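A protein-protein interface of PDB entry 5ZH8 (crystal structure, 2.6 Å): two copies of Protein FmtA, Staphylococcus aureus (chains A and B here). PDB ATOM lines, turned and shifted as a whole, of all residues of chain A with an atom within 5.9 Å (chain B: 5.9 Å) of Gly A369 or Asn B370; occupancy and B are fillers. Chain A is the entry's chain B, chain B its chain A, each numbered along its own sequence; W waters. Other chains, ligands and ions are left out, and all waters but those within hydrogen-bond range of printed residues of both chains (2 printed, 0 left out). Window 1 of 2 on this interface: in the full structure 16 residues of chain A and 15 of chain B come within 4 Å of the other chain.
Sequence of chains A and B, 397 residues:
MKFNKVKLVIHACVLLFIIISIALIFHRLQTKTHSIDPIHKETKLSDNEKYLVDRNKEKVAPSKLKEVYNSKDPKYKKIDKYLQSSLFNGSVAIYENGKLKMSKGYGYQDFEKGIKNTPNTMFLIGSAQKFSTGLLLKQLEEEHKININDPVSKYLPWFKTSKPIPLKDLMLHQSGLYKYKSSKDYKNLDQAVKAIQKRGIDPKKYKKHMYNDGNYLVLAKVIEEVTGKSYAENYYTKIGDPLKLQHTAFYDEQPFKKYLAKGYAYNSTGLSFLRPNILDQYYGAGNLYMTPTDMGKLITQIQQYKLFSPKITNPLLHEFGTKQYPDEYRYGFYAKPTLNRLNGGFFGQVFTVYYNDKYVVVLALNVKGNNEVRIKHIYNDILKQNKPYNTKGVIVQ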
ATOM      1  N   TYR A 266       1.205  24.572 -27.560  1.00  0.00           N
ATOM      2  CA  TYR A 266       2.070  23.768 -28.411  1.00  0.00           C
ATOM      3  C   TYR A 266       1.613  22.349 -28.134  1.00  0.00           C
ATOM      4  O   TYR A 266       1.842  21.831 -27.041  1.00  0.00           O
ATOM      5  CB  TYR A 266       3.536  23.945 -28.020  1.00  0.00           C
ATOM      6  CG  TYR A 266       3.819  25.218 -27.256  1.00  0.00           C
ATOM      7  CD1 TYR A 266       3.272  25.433 -25.998  1.00  0.00           C
ATOM      8  CD2 TYR A 266       4.634  26.207 -27.793  1.00  0.00           C
ATOM      9  CE1 TYR A 266       3.528  26.596 -25.296  1.00  0.00           C
ATOM     10  CE2 TYR A 266       4.895  27.373 -27.098  1.00  0.00           C
ATOM     11  CZ  TYR A 266       4.340  27.562 -25.851  1.00  0.00           C
ATOM     12  OH  TYR A 266       4.598  28.721 -25.156  1.00  0.00           O
ATOM     13  N   VAL A 350      -6.013  30.779 -19.851  1.00  0.00           N
ATOM     14  CA  VAL A 350      -6.423  30.423 -18.505  1.00  0.00           C
ATOM     15  C   VAL A 350      -6.572  31.708 -17.712  1.00  0.00           C
ATOM     16  O   VAL A 350      -5.641  32.507 -17.638  1.00  0.00           O
ATOM     17  CB  VAL A 350      -5.406  29.513 -17.787  1.00  0.00           C
ATOM     18  CG1 VAL A 350      -6.077  28.807 -16.620  1.00  0.00           C
ATOM     19  CG2 VAL A 350      -4.789  28.497 -18.742  1.00  0.00           C
ATOM     20  N   LEU A 365      -3.395  33.939 -18.340  1.00  0.00           N
ATOM     21  CA  LEU A 365      -2.362  33.238 -19.076  1.00  0.00           C
ATOM     22  C   LEU A 365      -2.866  32.902 -20.478  1.00  0.00           C
ATOM     23  O   LEU A 365      -3.871  32.208 -20.617  1.00  0.00           O
ATOM     24  CB  LEU A 365      -2.020  31.962 -18.321  1.00  0.00           C
ATOM     25  CG  LEU A 365      -0.854  31.118 -18.824  1.00  0.00           C
ATOM     26  CD1 LEU A 365       0.481  31.842 -18.666  1.00  0.00           C
ATOM     27  CD2 LEU A 365      -0.838  29.783 -18.087  1.00  0.00           C
ATOM     28  N   VAL A 367      -0.708  31.564 -22.983  1.00  0.00           N
ATOM     29  CA  VAL A 367      -0.056  30.345 -23.456  1.00  0.00           C
ATOM     30  C   VAL A 367      -0.432  29.253 -22.466  1.00  0.00           C
ATOM     31  O   VAL A 367      -0.101  29.337 -21.283  1.00  0.00           O
ATOM     32  CB  VAL A 367       1.476  30.481 -23.539  1.00  0.00           C
ATOM     33  CG1 VAL A 367       2.097  29.207 -24.099  1.00  0.00           C
ATOM     34  CG2 VAL A 367       1.856  31.669 -24.411  1.00  0.00           C
ATOM     35  N   LYS A 368      -1.130  28.231 -22.953  1.00  0.00           N
ATOM     36  CA  LYS A 368      -1.713  27.226 -22.071  1.00  0.00           C
ATOM     37  C   LYS A 368      -0.648  26.569 -21.208  1.00  0.00           C
ATOM     38  O   LYS A 368       0.434  26.230 -21.685  1.00  0.00           O
ATOM     39  CB  LYS A 368      -2.468  26.156 -22.864  1.00  0.00           C
ATOM     40  CG  LYS A 368      -3.329  25.263 -21.982  1.00  0.00           C
ATOM     41  CD  LYS A 368      -4.274  24.409 -22.793  1.00  0.00           C
ATOM     42  CE  LYS A 368      -5.113  23.536 -21.880  1.00  0.00           C
ATOM     43  NZ  LYS A 368      -6.040  22.674 -22.665  1.00  0.00           N
ATOM     44  N   GLY A 369      -0.975  26.394 -19.937  1.00  0.00           N
ATOM     45  CA  GLY A 369      -0.070  25.786 -18.986  1.00  0.00           C
ATOM     46  C   GLY A 369      -0.701  25.807 -17.618  1.00  0.00           C
ATOM     47  O   GLY A 369      -1.895  26.086 -17.481  1.00  0.00           O
ATOM     48  N   ASN A 370       0.104  25.523 -16.604  1.00  0.00           N
ATOM     49  CA  ASN A 370      -0.402  25.409 -15.249  1.00  0.00           C
ATOM     50  C   ASN A 370      -0.490  26.782 -14.573  1.00  0.00           C
ATOM     51  O   ASN A 370       0.493  27.283 -14.034  1.00  0.00           O
ATOM     52  CB  ASN A 370       0.488  24.463 -14.444  1.00  0.00           C
ATOM     53  CG  ASN A 370      -0.164  24.008 -13.166  1.00  0.00           C
ATOM     54  OD1 ASN A 370      -1.079  24.655 -12.662  1.00  0.00           O
ATOM     55  ND2 ASN A 370       0.297  22.886 -12.636  1.00  0.00           N
ATOM     56  N   ASN A 371      -1.673  27.385 -14.606  1.00  0.00           N
ATOM     57  CA  ASN A 371      -1.875  28.690 -13.990  1.00  0.00           C
ATOM     58  C   ASN A 371      -2.107  28.565 -12.481  1.00  0.00           C
ATOM     59  O   ASN A 371      -1.815  29.498 -11.732  1.00  0.00           O
ATOM     60  CB  ASN A 371      -3.052  29.418 -14.655  1.00  0.00           C
ATOM     61  CG  ASN A 371      -2.958  30.934 -14.525  1.00  0.00           C
ATOM     62  OD1 ASN A 371      -1.885  31.522 -14.689  1.00  0.00           O
ATOM     63  ND2 ASN A 371      -4.091  31.577 -14.240  1.00  0.00           N
ATOM     64  N   GLU A 372      -2.604  27.411 -12.031  1.00  0.00           N
ATOM     65  CA  GLU A 372      -3.008  27.228 -10.628  1.00  0.00           C
ATOM     66  C   GLU A 372      -1.814  27.221  -9.698  1.00  0.00           C
ATOM     67  O   GLU A 372      -1.856  27.801  -8.620  1.00  0.00           O
ATOM     68  CB  GLU A 372      -3.763  25.914 -10.442  1.00  0.00           C
ATOM     69  CG  GLU A 372      -4.605  25.872  -9.170  1.00  0.00           C
ATOM     70  CD  GLU A 372      -5.962  26.501  -9.343  1.00  0.00           C
ATOM     71  OE1 GLU A 372      -6.457  26.491 -10.485  1.00  0.00           O
ATOM     72  OE2 GLU A 372      -6.549  26.996  -8.354  1.00  0.00           O
ATOM     73  N   LEU B 365       7.618  15.734 -16.490  1.00  0.00           N
ATOM     74  CA  LEU B 365       6.750  16.535 -15.652  1.00  0.00           C
ATOM     75  C   LEU B 365       5.528  15.717 -15.236  1.00  0.00           C
ATOM     76  O   LEU B 365       4.782  15.259 -16.091  1.00  0.00           O
ATOM     77  CB  LEU B 365       6.323  17.764 -16.452  1.00  0.00           C
ATOM     78  CG  LEU B 365       5.506  18.830 -15.742  1.00  0.00           C
ATOM     79  CD1 LEU B 365       6.339  19.544 -14.684  1.00  0.00           C
ATOM     80  CD2 LEU B 365       4.977  19.804 -16.783  1.00  0.00           C
ATOM     81  N   LYS B 368       0.643  18.307 -14.542  1.00  0.00           N
ATOM     82  CA  LYS B 368       0.379  18.755 -15.903  1.00  0.00           C
ATOM     83  C   LYS B 368       0.593  20.254 -16.043  1.00  0.00           C
ATOM     84  O   LYS B 368       0.189  21.041 -15.181  1.00  0.00           O
ATOM     85  CB  LYS B 368      -1.042  18.401 -16.321  1.00  0.00           C
ATOM     86  CG  LYS B 368      -1.309  18.568 -17.805  1.00  0.00           C
ATOM     87  CD  LYS B 368      -2.714  18.071 -18.138  1.00  0.00           C
ATOM     88  CE  LYS B 368      -2.977  18.067 -19.635  1.00  0.00           C
ATOM     89  NZ  LYS B 368      -2.719  19.400 -20.259  1.00  0.00           N
ATOM     90  N   GLY B 369       1.232  20.634 -17.142  1.00  0.00           N
ATOM     91  CA  GLY B 369       1.528  22.028 -17.416  1.00  0.00           C
ATOM     92  C   GLY B 369       2.331  22.141 -18.685  1.00  0.00           C
ATOM     93  O   GLY B 369       2.464  21.180 -19.424  1.00  0.00           O
ATOM     94  N   ASN B 370       2.875  23.324 -18.931  1.00  0.00           N
ATOM     95  CA  ASN B 370       3.601  23.594 -20.162  1.00  0.00           C
ATOM     96  C   ASN B 370       5.055  23.137 -20.044  1.00  0.00           C
ATOM     97  O   ASN B 370       5.914  23.856 -19.516  1.00  0.00           O
ATOM     98  CB  ASN B 370       3.522  25.082 -20.484  1.00  0.00           C
ATOM     99  CG  ASN B 370       3.957  25.399 -21.893  1.00  0.00           C
ATOM    100  OD1 ASN B 370       4.662  24.619 -22.530  1.00  0.00           O
ATOM    101  ND2 ASN B 370       3.537  26.558 -22.387  1.00  0.00           N
ATOM    102  N   ASN B 371       5.336  21.939 -20.543  1.00  0.00           N
ATOM    103  CA  ASN B 371       6.692  21.406 -20.491  1.00  0.00           C
ATOM    104  C   ASN B 371       7.562  21.966 -21.631  1.00  0.00           C
ATOM    105  O   ASN B 371       8.781  22.035 -21.507  1.00  0.00           O
ATOM    106  CB  ASN B 371       6.655  19.870 -20.535  1.00  0.00           C
ATOM    107  CG  ASN B 371       7.883  19.235 -19.910  1.00  0.00           C
ATOM    108  OD1 ASN B 371       8.352  19.669 -18.849  1.00  0.00           O
ATOM    109  ND2 ASN B 371       8.407  18.196 -20.557  1.00  0.00           N
ATOM    110  N   GLU B 372       6.928  22.367 -22.733  1.00  0.00           N
ATOM    111  CA  GLU B 372       7.652  22.750 -23.957  1.00  0.00           C
ATOM    112  C   GLU B 372       8.406  24.057 -23.772  1.00  0.00           C
ATOM    113  O   GLU B 372       9.535  24.196 -24.224  1.00  0.00           O
ATOM    114  CB  GLU B 372       6.697  22.893 -25.136  1.00  0.00           C
ATOM    115  CG  GLU B 372       7.393  22.812 -26.484  1.00  0.00           C
ATOM    116  CD  GLU B 372       7.588  21.384 -26.984  1.00  0.00           C
ATOM    117  OE1 GLU B 372       6.840  20.497 -26.548  1.00  0.00           O
ATOM    118  OE2 GLU B 372       8.474  21.147 -27.835  1.00  0.00           O
ATOM    119  N   VAL B 373       7.767  25.013 -23.109  1.00  0.00           N
ATOM    120  CA  VAL B 373       8.404  26.279 -22.806  1.00  0.00           C
ATOM    121  C   VAL B 373       9.645  26.026 -21.960  1.00  0.00           C
ATOM    122  O   VAL B 373      10.665  26.690 -22.144  1.00  0.00           O
ATOM    123  CB  VAL B 373       7.440  27.247 -22.078  1.00  0.00           C
ATOM    124  CG1 VAL B 373       8.194  28.436 -21.505  1.00  0.00           C
ATOM    125  CG2 VAL B 373       6.356  27.742 -23.027  1.00  0.00           C
ATOM    126  N   ARG B 374       9.563  25.057 -21.053  1.00  0.00           N
ATOM    127  CA  ARG B 374      10.681  24.771 -20.153  1.00  0.00           C
ATOM    128  C   ARG B 374      11.861  24.186 -20.913  1.00  0.00           C
ATOM    129  O   ARG B 374      12.977  24.681 -20.812  1.00  0.00           O
ATOM    130  CB  ARG B 374      10.271  23.806 -19.032  1.00  0.00           C
ATOM    131  CG  ARG B 374       9.139  24.285 -18.133  1.00  0.00           C
ATOM    132  CD  ARG B 374       8.735  23.172 -17.177  1.00  0.00           C
ATOM    133  NE  ARG B 374       7.806  23.600 -16.129  1.00  0.00           N
ATOM    134  CZ  ARG B 374       8.146  24.327 -15.071  1.00  0.00           C
ATOM    135  NH1 ARG B 374       9.392  24.752 -14.915  1.00  0.00           N
ATOM    136  NH2 ARG B 374       7.230  24.648 -14.171  1.00  0.00           N
HETATM  137  O   HOH W   1       3.294  25.440 -16.699  1.00  0.00           O
HETATM  138  O   HOH W   2       2.836  21.852 -14.021  1.00  0.00           O
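The side-chain amide oxygen (OD1) of Asn B370 sits at hydrogen-bond distance from the backbone NH (N) of Glu B372 (3.2 Å).
The side-chain amide oxygen (OD1) of Asn B370 lies within hydrogen-bond range of the backbone NH (N) of Val B373, at 3.2 Å.
The side-chain amide oxygen (OD1) of Asn A370 sits at hydrogen-bond distance from the backbone NH (N) of Glu A372, 3.2 Å away.
ND2 of Asn A370 is in hydrogen-bond range of O of Lys B368 (3.1 Å).
ND2 of Asn B370 sits at hydrogen-bond distance from O of Lys A368, 3.2 Å away.
Lys A368 touches Asn B370, and with the chains exchanged Asn A370 touches Lys B368.
Gly A369 touches Asn B370, and with the chains exchanged Asn A370 touches Gly B369.
6 positions are printed for both chains.
Among the printed residues, merely in contact across the chains: Tyr A266 with Asn B370, Tyr A266 with Val B373, Val A367 with Asn B370, Gly A369 with Asn B370 and Asn A370 with Gly B369.
Gly A369 touches just one residue of chain B: Asn B370.
Of the printed residues of chain A, Asn B370 touches Tyr A266, Val A367, Lys A368 and Gly A369.
Of the printed residues of chain B, Tyr A266 touches Asn B370 (2.9 Å) and Val B373 (2.9 Å).
Of the printed residues of chain A, Val B373 touches Tyr A266.
Printed residues of chain B within 4 Å of Asn A370: Lys B368 and Gly B369.
Of the printed residues of chain A, Lys B368 touches Asn A370 (3.1 Å).
Of the printed residues of chain B, Val A367 touches Asn B370 (3.5 Å).
Asn B371 touches none of the printed residues of chain A.
Arg B374 touches none of the printed residues of chain A.
The nearest residue of chain A that does not touch Asn B370 is Asn A370 (4.2 Å).
The nearest printed residue of chain B that does not touch Lys A368 is Lys B368 (5.0 Å).
Water W2 bridges the backbone carbonyl oxygen (O) of Lys B368 (3.0 Å) and the side-chain amide nitrogen (ND2) of Asn A370 (3.1 Å).
Water W1 lies within hydrogen-bond range of the backbone NH of Asn B370 (3.1 Å) and the backbone NH of Asn A370 (3.2 Å).
Printed residues of chain A that touch a printed residue of chain B: Tyr A266, Val A367, Lys A368, Gly A369 and Asn A370.
Hydrophobic or aromatic side chains of chain A within 4 Å of the printed part of chain B: Tyr A266 and Val A367.
Hydrophobic or aromatic side chains of chain B that line the printed part of chain A: Val B373.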
